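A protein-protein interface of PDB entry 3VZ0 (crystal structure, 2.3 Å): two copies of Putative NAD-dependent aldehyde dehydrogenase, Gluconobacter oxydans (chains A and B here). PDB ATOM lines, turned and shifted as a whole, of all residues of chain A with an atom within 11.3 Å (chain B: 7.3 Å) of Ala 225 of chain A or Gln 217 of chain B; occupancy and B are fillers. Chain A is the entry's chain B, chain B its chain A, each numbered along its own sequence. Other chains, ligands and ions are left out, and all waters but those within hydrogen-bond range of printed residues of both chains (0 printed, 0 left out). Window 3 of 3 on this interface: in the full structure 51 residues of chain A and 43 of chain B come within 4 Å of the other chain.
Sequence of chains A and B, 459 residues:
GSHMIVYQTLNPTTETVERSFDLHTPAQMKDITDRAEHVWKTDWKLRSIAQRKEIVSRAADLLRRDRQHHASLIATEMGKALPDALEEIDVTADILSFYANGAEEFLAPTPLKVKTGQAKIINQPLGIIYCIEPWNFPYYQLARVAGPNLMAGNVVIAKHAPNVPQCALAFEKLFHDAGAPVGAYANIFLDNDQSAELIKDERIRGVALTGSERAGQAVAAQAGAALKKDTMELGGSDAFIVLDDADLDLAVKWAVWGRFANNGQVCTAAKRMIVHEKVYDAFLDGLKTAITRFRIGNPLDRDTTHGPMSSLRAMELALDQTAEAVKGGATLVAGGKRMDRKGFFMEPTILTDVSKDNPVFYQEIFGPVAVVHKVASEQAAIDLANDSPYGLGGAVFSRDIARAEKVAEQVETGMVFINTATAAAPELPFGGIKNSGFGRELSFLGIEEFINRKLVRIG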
ATOM      1  N   ALA A 196      23.442  27.668  12.429  1.00  0.00           N
ATOM      2  CA  ALA A 196      23.880  27.069  11.181  1.00  0.00           C
ATOM      3  C   ALA A 196      25.057  27.828  10.584  1.00  0.00           C
ATOM      4  O   ALA A 196      25.982  27.197  10.064  1.00  0.00           O
ATOM      5  CB  ALA A 196      22.725  26.964  10.171  1.00  0.00           C
ATOM      6  N   GLU A 197      25.001  29.166  10.638  1.00  0.00           N
ATOM      7  CA  GLU A 197      26.064  30.031  10.129  1.00  0.00           C
ATOM      8  C   GLU A 197      27.366  29.870  10.938  1.00  0.00           C
ATOM      9  O   GLU A 197      28.460  29.927  10.376  1.00  0.00           O
ATOM     10  CB  GLU A 197      25.597  31.507  10.036  1.00  0.00           C
ATOM     11  CG  GLU A 197      24.771  31.815   8.756  1.00  0.00           C
ATOM     12  CD  GLU A 197      24.090  33.208   8.721  1.00  0.00           C
ATOM     13  OE1 GLU A 197      23.432  33.620   9.723  1.00  0.00           O
ATOM     14  OE2 GLU A 197      24.178  33.890   7.656  1.00  0.00           O
ATOM     15  N   LEU A 198      27.245  29.661  12.250  1.00  0.00           N
ATOM     16  CA  LEU A 198      28.412  29.355  13.083  1.00  0.00           C
ATOM     17  C   LEU A 198      29.036  28.004  12.715  1.00  0.00           C
ATOM     18  O   LEU A 198      30.265  27.845  12.753  1.00  0.00           O
ATOM     19  CB  LEU A 198      28.069  29.370  14.575  1.00  0.00           C
ATOM     20  CG  LEU A 198      29.258  29.267  15.555  1.00  0.00           C
ATOM     21  CD1 LEU A 198      30.246  30.435  15.391  1.00  0.00           C
ATOM     22  CD2 LEU A 198      28.776  29.186  16.999  1.00  0.00           C
ATOM     23  N   ILE A 199      28.195  27.028  12.374  1.00  0.00           N
ATOM     24  CA  ILE A 199      28.730  25.721  11.985  1.00  0.00           C
ATOM     25  C   ILE A 199      29.558  25.820  10.700  1.00  0.00           C
ATOM     26  O   ILE A 199      30.611  25.192  10.610  1.00  0.00           O
ATOM     27  CB  ILE A 199      27.635  24.607  11.968  1.00  0.00           C
ATOM     28  CG1 ILE A 199      27.352  24.181  13.413  1.00  0.00           C
ATOM     29  CG2 ILE A 199      28.051  23.372  11.102  1.00  0.00           C
ATOM     30  CD1 ILE A 199      25.975  23.606  13.640  1.00  0.00           C
ATOM     31  N   LYS A 200      29.094  26.636   9.746  1.00  0.00           N
ATOM     32  CA  LYS A 200      29.804  26.915   8.492  1.00  0.00           C
ATOM     33  C   LYS A 200      31.157  27.613   8.663  1.00  0.00           C
ATOM     34  O   LYS A 200      32.038  27.450   7.827  1.00  0.00           O
ATOM     35  CB  LYS A 200      28.949  27.777   7.548  1.00  0.00           C
ATOM     36  CG  LYS A 200      27.729  27.100   6.949  1.00  0.00           C
ATOM     37  CD  LYS A 200      27.107  27.987   5.887  1.00  0.00           C
ATOM     38  CE  LYS A 200      25.659  27.590   5.573  1.00  0.00           C
ATOM     39  NZ  LYS A 200      25.022  28.556   4.594  1.00  0.00           N
ATOM     40  N   ASP A 201      31.316  28.404   9.723  1.00  0.00           N
ATOM     41  CA  ASP A 201      32.566  29.135   9.970  1.00  0.00           C
ATOM     42  C   ASP A 201      33.741  28.154  10.023  1.00  0.00           C
ATOM     43  O   ASP A 201      33.745  27.264  10.849  1.00  0.00           O
ATOM     44  CB  ASP A 201      32.458  29.939  11.276  1.00  0.00           C
ATOM     45  CG  ASP A 201      33.585  30.960  11.451  1.00  0.00           C
ATOM     46  OD1 ASP A 201      34.772  30.602  11.347  1.00  0.00           O
ATOM     47  OD2 ASP A 201      33.283  32.139  11.721  1.00  0.00           O
ATOM     48  N   GLU A 202      34.728  28.353   9.141  1.00  0.00           N
ATOM     49  CA  GLU A 202      35.929  27.498   9.006  1.00  0.00           C
ATOM     50  C   GLU A 202      36.700  27.345  10.318  1.00  0.00           C
ATOM     51  O   GLU A 202      37.435  26.377  10.497  1.00  0.00           O
ATOM     52  CB  GLU A 202      36.909  28.053   7.939  1.00  0.00           C
ATOM     53  CG  GLU A 202      36.316  28.976   6.833  1.00  0.00           C
ATOM     54  CD  GLU A 202      35.676  30.279   7.363  1.00  0.00           C
ATOM     55  OE1 GLU A 202      36.327  31.033   8.142  1.00  0.00           O
ATOM     56  OE2 GLU A 202      34.510  30.546   7.000  1.00  0.00           O
ATOM     57  N   ILE A 204      35.377  26.951  13.446  1.00  0.00           N
ATOM     58  CA  ILE A 204      34.760  25.899  14.262  1.00  0.00           C
ATOM     59  C   ILE A 204      35.236  24.554  13.726  1.00  0.00           C
ATOM     60  O   ILE A 204      35.016  24.253  12.556  1.00  0.00           O
ATOM     61  CB  ILE A 204      33.207  25.965  14.200  1.00  0.00           C
ATOM     62  CG1 ILE A 204      32.680  27.329  14.694  1.00  0.00           C
ATOM     63  CG2 ILE A 204      32.555  24.759  14.907  1.00  0.00           C
ATOM     64  CD1 ILE A 204      33.134  27.752  16.076  1.00  0.00           C
ATOM     65  N   ARG A 205      35.912  23.764  14.561  1.00  0.00           N
ATOM     66  CA  ARG A 205      36.576  22.536  14.082  1.00  0.00           C
ATOM     67  C   ARG A 205      35.857  21.272  14.516  1.00  0.00           C
ATOM     68  O   ARG A 205      36.248  20.177  14.149  1.00  0.00           O
ATOM     69  CB  ARG A 205      38.067  22.483  14.487  1.00  0.00           C
ATOM     70  CG  ARG A 205      38.972  23.593  13.901  1.00  0.00           C
ATOM     71  CD  ARG A 205      38.672  23.942  12.432  1.00  0.00           C
ATOM     72  NE  ARG A 205      38.637  22.751  11.586  1.00  0.00           N
ATOM     73  CZ  ARG A 205      37.939  22.616  10.456  1.00  0.00           C
ATOM     74  NH1 ARG A 205      37.201  23.604   9.952  1.00  0.00           N
ATOM     75  NH2 ARG A 205      37.999  21.460   9.817  1.00  0.00           N
ATOM     76  N   VAL A 207      31.689  19.891  16.308  1.00  0.00           N
ATOM     77  CA  VAL A 207      30.390  20.142  16.914  1.00  0.00           C
ATOM     78  C   VAL A 207      29.987  18.969  17.785  1.00  0.00           C
ATOM     79  O   VAL A 207      29.934  17.840  17.323  1.00  0.00           O
ATOM     80  CB  VAL A 207      29.278  20.360  15.859  1.00  0.00           C
ATOM     81  CG1 VAL A 207      28.031  20.886  16.527  1.00  0.00           C
ATOM     82  CG2 VAL A 207      29.750  21.306  14.744  1.00  0.00           C
ATOM     83  N   GLY A 216      19.540  16.811  16.236  1.00  0.00           N
ATOM     84  CA  GLY A 216      20.651  16.002  15.727  1.00  0.00           C
ATOM     85  C   GLY A 216      20.757  15.919  14.211  1.00  0.00           C
ATOM     86  O   GLY A 216      21.816  16.242  13.649  1.00  0.00           O
ATOM     87  N   GLN A 217      19.662  15.516  13.561  1.00  0.00           N
ATOM     88  CA  GLN A 217      19.604  15.383  12.098  1.00  0.00           C
ATOM     89  C   GLN A 217      20.018  16.649  11.346  1.00  0.00           C
ATOM     90  O   GLN A 217      20.662  16.572  10.294  1.00  0.00           O
ATOM     91  CB  GLN A 217      18.186  14.956  11.631  1.00  0.00           C
ATOM     92  CG  GLN A 217      17.764  13.544  12.056  1.00  0.00           C
ATOM     93  CD  GLN A 217      16.350  13.134  11.594  1.00  0.00           C
ATOM     94  OE1 GLN A 217      15.637  13.892  10.917  1.00  0.00           O
ATOM     95  NE2 GLN A 217      15.945  11.924  11.974  1.00  0.00           N
ATOM     96  N   ALA A 218      19.593  17.800  11.865  1.00  0.00           N
ATOM     97  CA  ALA A 218      19.847  19.094  11.236  1.00  0.00           C
ATOM     98  C   ALA A 218      21.288  19.525  11.455  1.00  0.00           C
ATOM     99  O   ALA A 218      21.954  19.980  10.527  1.00  0.00           O
ATOM    100  CB  ALA A 218      18.905  20.146  11.785  1.00  0.00           C
ATOM    101  N   VAL A 219      21.771  19.390  12.684  1.00  0.00           N
ATOM    102  CA  VAL A 219      23.133  19.820  13.009  1.00  0.00           C
ATOM    103  C   VAL A 219      24.211  18.916  12.383  1.00  0.00           C
ATOM    104  O   VAL A 219      25.238  19.421  11.888  1.00  0.00           O
ATOM    105  CB  VAL A 219      23.337  19.956  14.524  1.00  0.00           C
ATOM    106  CG1 VAL A 219      24.856  20.108  14.884  1.00  0.00           C
ATOM    107  CG2 VAL A 219      22.522  21.125  15.069  1.00  0.00           C
ATOM    108  N   ALA A 220      23.975  17.601  12.407  1.00  0.00           N
ATOM    109  CA  ALA A 220      24.917  16.612  11.831  1.00  0.00           C
ATOM    110  C   ALA A 220      25.042  16.759  10.313  1.00  0.00           C
ATOM    111  O   ALA A 220      26.114  16.568   9.761  1.00  0.00           O
ATOM    112  CB  ALA A 220      24.521  15.195  12.192  1.00  0.00           C
ATOM    113  N   ALA A 221      23.937  17.094   9.655  1.00  0.00           N
ATOM    114  CA  ALA A 221      23.914  17.402   8.227  1.00  0.00           C
ATOM    115  C   ALA A 221      24.768  18.630   7.916  1.00  0.00           C
ATOM    116  O   ALA A 221      25.601  18.593   7.003  1.00  0.00           O
ATOM    117  CB  ALA A 221      22.493  17.653   7.798  1.00  0.00           C
ATOM    118  N   GLN A 222      24.522  19.706   8.671  1.00  0.00           N
ATOM    119  CA  GLN A 222      25.305  20.951   8.676  1.00  0.00           C
ATOM    120  C   GLN A 222      26.811  20.770   8.900  1.00  0.00           C
ATOM    121  O   GLN A 222      27.612  21.382   8.187  1.00  0.00           O
ATOM    122  CB  GLN A 222      24.762  21.929   9.738  1.00  0.00           C
ATOM    123  CG  GLN A 222      23.430  22.609   9.394  1.00  0.00           C
ATOM    124  CD  GLN A 222      22.717  23.190  10.627  1.00  0.00           C
ATOM    125  OE1 GLN A 222      23.284  23.268  11.719  1.00  0.00           O
ATOM    126  NE2 GLN A 222      21.467  23.590  10.450  1.00  0.00           N
ATOM    127  N   ALA A 223      27.186  19.977   9.908  1.00  0.00           N
ATOM    128  CA  ALA A 223      28.594  19.710  10.218  1.00  0.00           C
ATOM    129  C   ALA A 223      29.247  18.889   9.101  1.00  0.00           C
ATOM    130  O   ALA A 223      30.371  19.200   8.677  1.00  0.00           O
ATOM    131  CB  ALA A 223      28.745  19.003  11.571  1.00  0.00           C
ATOM    132  N   GLY A 224      28.546  17.853   8.625  1.00  0.00           N
ATOM    133  CA  GLY A 224      29.003  17.070   7.477  1.00  0.00           C
ATOM    134  C   GLY A 224      29.251  17.970   6.278  1.00  0.00           C
ATOM    135  O   GLY A 224      30.308  17.887   5.643  1.00  0.00           O
ATOM    136  N   ALA A 225      28.286  18.843   5.976  1.00  0.00           N
ATOM    137  CA  ALA A 225      28.379  19.713   4.790  1.00  0.00           C
ATOM    138  C   ALA A 225      29.522  20.730   4.917  1.00  0.00           C
ATOM    139  O   ALA A 225      30.043  21.222   3.918  1.00  0.00           O
ATOM    140  CB  ALA A 225      27.042  20.430   4.522  1.00  0.00           C
ATOM    141  N   ALA A 226      29.898  21.033   6.153  1.00  0.00           N
ATOM    142  CA  ALA A 226      30.980  21.960   6.417  1.00  0.00           C
ATOM    143  C   ALA A 226      32.299  21.204   6.651  1.00  0.00           C
ATOM    144  O   ALA A 226      33.310  21.803   7.013  1.00  0.00           O
ATOM    145  CB  ALA A 226      30.623  22.843   7.607  1.00  0.00           C
ATOM    146  N   LEU A 227      32.270  19.892   6.412  1.00  0.00           N
ATOM    147  CA  LEU A 227      33.414  18.982   6.579  1.00  0.00           C
ATOM    148  C   LEU A 227      34.066  19.031   7.977  1.00  0.00           C
ATOM    149  O   LEU A 227      35.275  19.235   8.118  1.00  0.00           O
ATOM    150  CB  LEU A 227      34.463  19.199   5.467  1.00  0.00           C
ATOM    151  CG  LEU A 227      34.100  19.012   3.987  1.00  0.00           C
ATOM    152  CD1 LEU A 227      35.357  19.243   3.114  1.00  0.00           C
ATOM    153  CD2 LEU A 227      33.479  17.643   3.693  1.00  0.00           C
ATOM    154  N   LYS A 228      33.254  18.840   9.007  1.00  0.00           N
ATOM    155  CA  LYS A 228      33.749  18.828  10.385  1.00  0.00           C
ATOM    156  C   LYS A 228      33.277  17.588  11.087  1.00  0.00           C
ATOM    157  O   LYS A 228      32.216  17.066  10.763  1.00  0.00           O
ATOM    158  CB  LYS A 228      33.230  20.039  11.165  1.00  0.00           C
ATOM    159  CG  LYS A 228      33.879  21.321  10.759  1.00  0.00           C
ATOM    160  CD  LYS A 228      33.009  22.520  11.040  1.00  0.00           C
ATOM    161  CE  LYS A 228      33.367  23.547  10.012  1.00  0.00           C
ATOM    162  NZ  LYS A 228      33.252  24.927  10.488  1.00  0.00           N
ATOM    163  N   LYS A 229      34.055  17.159  12.076  1.00  0.00           N
ATOM    164  CA  LYS A 229      33.636  16.117  12.992  1.00  0.00           C
ATOM    165  C   LYS A 229      32.479  16.594  13.876  1.00  0.00           C
ATOM    166  O   LYS A 229      32.518  17.683  14.447  1.00  0.00           O
ATOM    167  CB  LYS A 229      34.819  15.645  13.855  1.00  0.00           C
ATOM    168  CG  LYS A 229      34.404  14.639  14.918  1.00  0.00           C
ATOM    169  CD  LYS A 229      35.406  13.503  15.086  1.00  0.00           C
ATOM    170  CE  LYS A 229      34.805  12.403  15.959  1.00  0.00           C
ATOM    171  NZ  LYS A 229      35.862  11.573  16.615  1.00  0.00           N
ATOM    172  N   ASP A 230      31.438  15.774  13.966  1.00  0.00           N
ATOM    173  CA  ASP A 230      30.352  16.018  14.909  1.00  0.00           C
ATOM    174  C   ASP A 230      30.254  14.859  15.889  1.00  0.00           C
ATOM    175  O   ASP A 230      30.753  13.765  15.622  1.00  0.00           O
ATOM    176  CB  ASP A 230      29.018  16.299  14.205  1.00  0.00           C
ATOM    177  CG  ASP A 230      28.591  15.186  13.264  1.00  0.00           C
ATOM    178  OD1 ASP A 230      28.187  15.497  12.121  1.00  0.00           O
ATOM    179  OD2 ASP A 230      28.653  14.000  13.652  1.00  0.00           O
ATOM    180  N   MET A 232      27.277  13.075  18.543  1.00  0.00           N
ATOM    181  CA  MET A 232      25.821  13.076  18.692  1.00  0.00           C
ATOM    182  C   MET A 232      25.369  12.163  19.807  1.00  0.00           C
ATOM    183  O   MET A 232      25.686  10.969  19.820  1.00  0.00           O
ATOM    184  CB  MET A 232      25.136  12.633  17.399  1.00  0.00           C
ATOM    185  CG  MET A 232      25.416  13.519  16.218  1.00  0.00           C
ATOM    186  SD  MET A 232      24.296  15.095  16.221  1.00  0.00           S
ATOM    187  CE  MET A 232      25.666  16.463  15.822  1.00  0.00           C
ATOM    188  N   LEU B 209      34.296   6.975   3.336  1.00  0.00           N
ATOM    189  CA  LEU B 209      34.635   7.546   2.039  1.00  0.00           C
ATOM    190  C   LEU B 209      36.108   7.964   1.938  1.00  0.00           C
ATOM    191  O   LEU B 209      36.638   8.644   2.817  1.00  0.00           O
ATOM    192  CB  LEU B 209      33.715   8.737   1.687  1.00  0.00           C
ATOM    193  CG  LEU B 209      34.068   9.474   0.368  1.00  0.00           C
ATOM    194  CD1 LEU B 209      32.876   9.720  -0.507  1.00  0.00           C
ATOM    195  CD2 LEU B 209      34.777  10.798   0.612  1.00  0.00           C
ATOM    196  N   SER B 212      37.415  13.067  -3.013  1.00  0.00           N
ATOM    197  CA  SER B 212      37.566  14.521  -3.149  1.00  0.00           C
ATOM    198  C   SER B 212      36.675  15.269  -2.151  1.00  0.00           C
ATOM    199  O   SER B 212      35.673  14.724  -1.683  1.00  0.00           O
ATOM    200  CB  SER B 212      37.227  14.964  -4.587  1.00  0.00           C
ATOM    201  OG  SER B 212      35.821  14.968  -4.806  1.00  0.00           O
ATOM    202  N   GLU B 213      37.047  16.516  -1.849  1.00  0.00           N
ATOM    203  CA  GLU B 213      36.277  17.411  -0.975  1.00  0.00           C
ATOM    204  C   GLU B 213      34.798  17.458  -1.322  1.00  0.00           C
ATOM    205  O   GLU B 213      33.929  17.348  -0.451  1.00  0.00           O
ATOM    206  CB  GLU B 213      36.807  18.840  -1.095  1.00  0.00           C
ATOM    207  CG  GLU B 213      37.668  19.331   0.050  1.00  0.00           C
ATOM    208  CD  GLU B 213      37.738  20.858   0.071  1.00  0.00           C
ATOM    209  OE1 GLU B 213      36.755  21.500   0.515  1.00  0.00           O
ATOM    210  OE2 GLU B 213      38.765  21.418  -0.370  1.00  0.00           O
ATOM    211  N   ARG B 214      34.537  17.656  -2.609  1.00  0.00           N
ATOM    212  CA  ARG B 214      33.202  17.821  -3.155  1.00  0.00           C
ATOM    213  C   ARG B 214      32.377  16.581  -2.886  1.00  0.00           C
ATOM    214  O   ARG B 214      31.253  16.675  -2.380  1.00  0.00           O
ATOM    215  CB  ARG B 214      33.325  18.050  -4.652  1.00  0.00           C
ATOM    216  CG  ARG B 214      32.042  18.288  -5.386  1.00  0.00           C
ATOM    217  CD  ARG B 214      32.353  18.998  -6.689  1.00  0.00           C
ATOM    218  NE  ARG B 214      32.983  20.292  -6.416  1.00  0.00           N
ATOM    219  CZ  ARG B 214      33.886  20.875  -7.201  1.00  0.00           C
ATOM    220  NH1 ARG B 214      34.280  20.278  -8.327  1.00  0.00           N
ATOM    221  NH2 ARG B 214      34.397  22.054  -6.850  1.00  0.00           N
ATOM    222  N   ALA B 215      32.952  15.423  -3.218  1.00  0.00           N
ATOM    223  CA  ALA B 215      32.346  14.130  -2.933  1.00  0.00           C
ATOM    224  C   ALA B 215      32.133  13.997  -1.435  1.00  0.00           C
ATOM    225  O   ALA B 215      31.079  13.543  -0.994  1.00  0.00           O
ATOM    226  CB  ALA B 215      33.226  12.995  -3.460  1.00  0.00           C
ATOM    227  N   GLY B 216      33.123  14.419  -0.655  1.00  0.00           N
ATOM    228  CA  GLY B 216      33.044  14.333   0.811  1.00  0.00           C
ATOM    229  C   GLY B 216      31.922  15.171   1.404  1.00  0.00           C
ATOM    230  O   GLY B 216      31.204  14.708   2.301  1.00  0.00           O
ATOM    231  N   GLN B 217      31.773  16.397   0.893  1.00  0.00           N
ATOM    232  CA  GLN B 217      30.726  17.341   1.335  1.00  0.00           C
ATOM    233  C   GLN B 217      29.317  16.830   1.090  1.00  0.00           C
ATOM    234  O   GLN B 217      28.435  17.035   1.941  1.00  0.00           O
ATOM    235  CB  GLN B 217      30.857  18.706   0.634  1.00  0.00           C
ATOM    236  CG  GLN B 217      32.157  19.456   0.881  1.00  0.00           C
ATOM    237  CD  GLN B 217      32.232  20.760   0.119  1.00  0.00           C
ATOM    238  OE1 GLN B 217      31.647  21.753   0.531  1.00  0.00           O
ATOM    239  NE2 GLN B 217      32.958  20.767  -0.996  1.00  0.00           N
ATOM    240  N   ALA B 218      29.098  16.203  -0.077  1.00  0.00           N
ATOM    241  CA  ALA B 218      27.777  15.657  -0.421  1.00  0.00           C
ATOM    242  C   ALA B 218      27.442  14.471   0.481  1.00  0.00           C
ATOM    243  O   ALA B 218      26.372  14.423   1.098  1.00  0.00           O
ATOM    244  CB  ALA B 218      27.715  15.243  -1.895  1.00  0.00           C
ATOM    245  N   VAL B 219      28.387  13.543   0.571  1.00  0.00           N
ATOM    246  CA  VAL B 219      28.239  12.305   1.344  1.00  0.00           C
ATOM    247  C   VAL B 219      28.220  12.494   2.866  1.00  0.00           C
ATOM    248  O   VAL B 219      27.387  11.875   3.547  1.00  0.00           O
ATOM    249  CB  VAL B 219      29.328  11.286   0.963  1.00  0.00           C
ATOM    250  CG1 VAL B 219      29.268  10.078   1.896  1.00  0.00           C
ATOM    251  CG2 VAL B 219      29.149  10.864  -0.499  1.00  0.00           C
ATOM    252  N   ALA B 220      29.114  13.330   3.400  1.00  0.00           N
ATOM    253  CA  ALA B 220      29.111  13.582   4.850  1.00  0.00           C
ATOM    254  C   ALA B 220      27.797  14.222   5.318  1.00  0.00           C
ATOM    255  O   ALA B 220      27.240  13.821   6.350  1.00  0.00           O
ATOM    256  CB  ALA B 220      30.312  14.416   5.276  1.00  0.00           C
ATOM    257  N   ALA B 221      27.297  15.189   4.546  1.00  0.00           N
ATOM    258  CA  ALA B 221      25.971  15.773   4.794  1.00  0.00           C
ATOM    259  C   ALA B 221      24.844  14.739   4.760  1.00  0.00           C
ATOM    260  O   ALA B 221      23.924  14.802   5.573  1.00  0.00           O
ATOM    261  CB  ALA B 221      25.683  16.934   3.820  1.00  0.00           C
ATOM    262  N   GLN B 222      24.913  13.794   3.827  1.00  0.00           N
ATOM    263  CA  GLN B 222      23.934  12.698   3.748  1.00  0.00           C
ATOM    264  C   GLN B 222      24.000  11.771   4.970  1.00  0.00           C
ATOM    265  O   GLN B 222      22.967  11.389   5.537  1.00  0.00           O
ATOM    266  CB  GLN B 222      24.150  11.884   2.476  1.00  0.00           C
ATOM    267  CG  GLN B 222      23.633  12.554   1.214  1.00  0.00           C
ATOM    268  CD  GLN B 222      24.324  12.066  -0.054  1.00  0.00           C
ATOM    269  OE1 GLN B 222      24.958  11.011  -0.073  1.00  0.00           O
ATOM    270  NE2 GLN B 222      24.191  12.842  -1.130  1.00  0.00           N
ATOM    271  N   GLY B 224      25.308  12.481   7.955  1.00  0.00           N
ATOM    272  CA  GLY B 224      24.804  13.310   9.051  1.00  0.00           C
ATOM    273  C   GLY B 224      23.289  13.320   9.148  1.00  0.00           C
ATOM    274  O   GLY B 224      22.719  13.074  10.226  1.00  0.00           O
ATOM    275  N   MET B 232      35.796  10.340   6.657  1.00  0.00           N
ATOM    276  CA  MET B 232      36.082  11.074   5.428  1.00  0.00           C
ATOM    277  C   MET B 232      37.594  11.200   5.290  1.00  0.00           C
ATOM    278  O   MET B 232      38.246  11.756   6.174  1.00  0.00           O
ATOM    279  CB  MET B 232      35.404  12.457   5.478  1.00  0.00           C
ATOM    280  CG  MET B 232      33.892  12.399   5.623  1.00  0.00           C
ATOM    281  SD  MET B 232      32.950  11.709   4.023  1.00  0.00           S
ATOM    282  CE  MET B 232      31.766  10.363   4.795  1.00  0.00           C
ATOM    283  N   LEU B 234      40.040  12.733   2.571  1.00  0.00           N
ATOM    284  CA  LEU B 234      39.841  13.642   1.461  1.00  0.00           C
ATOM    285  C   LEU B 234      41.191  14.066   0.857  1.00  0.00           C
ATOM    286  O   LEU B 234      42.204  13.409   1.097  1.00  0.00           O
ATOM    287  CB  LEU B 234      38.968  14.810   1.929  1.00  0.00           C
ATOM    288  CG  LEU B 234      37.429  14.676   1.960  1.00  0.00           C
ATOM    289  CD1 LEU B 234      36.840  13.264   1.808  1.00  0.00           C
ATOM    290  CD2 LEU B 234      36.837  15.337   3.181  1.00  0.00           C
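Printed residues of chain A that touch a printed residue of chain B: Ala 220, Ala 221, Gly 224, Ala 225 and Leu 227. Of the 15 printed residues of chain B, 6 touch a printed residue of chain A. Hydrophobic or aromatic side chains of chain B within 4 Å of the printed part of chain A: Ala 220 and Ala 221. Along chain B the printed residues that touch a printed residue of chain A span positions 213 to 224. Among the printed residues, no Asp or Glu carboxylate lies within 4 Å of a Lys or Arg side-chain nitrogen of the other chain.
Of the printed residues of chain B, Ala 221 of chain A touches Ala 221 and Gly 224. Gly 224 of chain A touches two residues of chain B. Of chain B, only Gln 217 (3.8 Å) and Ala 221 (3.8 Å) come within 4 Å of Ala 225 of chain A. Of chain A, only Leu 227 (3.7 Å) comes within 4 Å of Glu 213 of chain B. No residue of chain A comes within 4 Å of Ala 215 of chain B. No residue of chain A comes within 4 Å of Ala 218 of chain B. No residue of chain A comes within 4 Å of Val 219 of chain B. Ala 220 of chain B touches just one residue of chain A: Gly 224 (3.5 Å). Of the printed residues of chain A, Gly 224 of chain B touches Ala 220 and Ala 221. Leu 234 of chain B touches none of the printed residues of chain A. The nearest residue of chain B that does not touch Ala 225 of chain A is Ala 220 of chain B (4.7 Å).
Ala 220 of chain A touches Gly 224 of chain B, and with the chains exchanged Gly 224 of chain A touches Ala 220 of chain B. Ala 221 of chain B touches its own counterpart, Ala 221 of chain A. Ala 221 of chain A touches Gly 224 of chain B, and with the chains exchanged Gly 224 of chain A touches Ala 221 of chain B. Of the 10 pairs that touch across the chains among the printed residues, 5 have their exchanged pair printed and touching as well.
Among the printed residues, merely in contact across the chains: Ala 220 of chain A with Gly 224 of chain B (3.4 Å), Gly 224 of chain A with Ala 220 of chain B (3.5 Å), Leu 227 of chain A with Gln 217 of chain B (3.5 Å), Ala 221 of chain A with Ala 221 of chain B (3.6 Å), Leu 227 of chain A with Gly 216 of chain B (3.7 Å), Leu 227 of chain A with Glu 213 of chain B (3.7 Å), Ala 225 of chain A with Gln 217 of chain B (3.8 Å), Gly 224 of chain A with Ala 221 of chain B (3.8 Å), Ala 225 of chain A with Ala 221 of chain B (3.8 Å) and Ala 221 of chain A with Gly 224 of chain B (3.9 Å).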
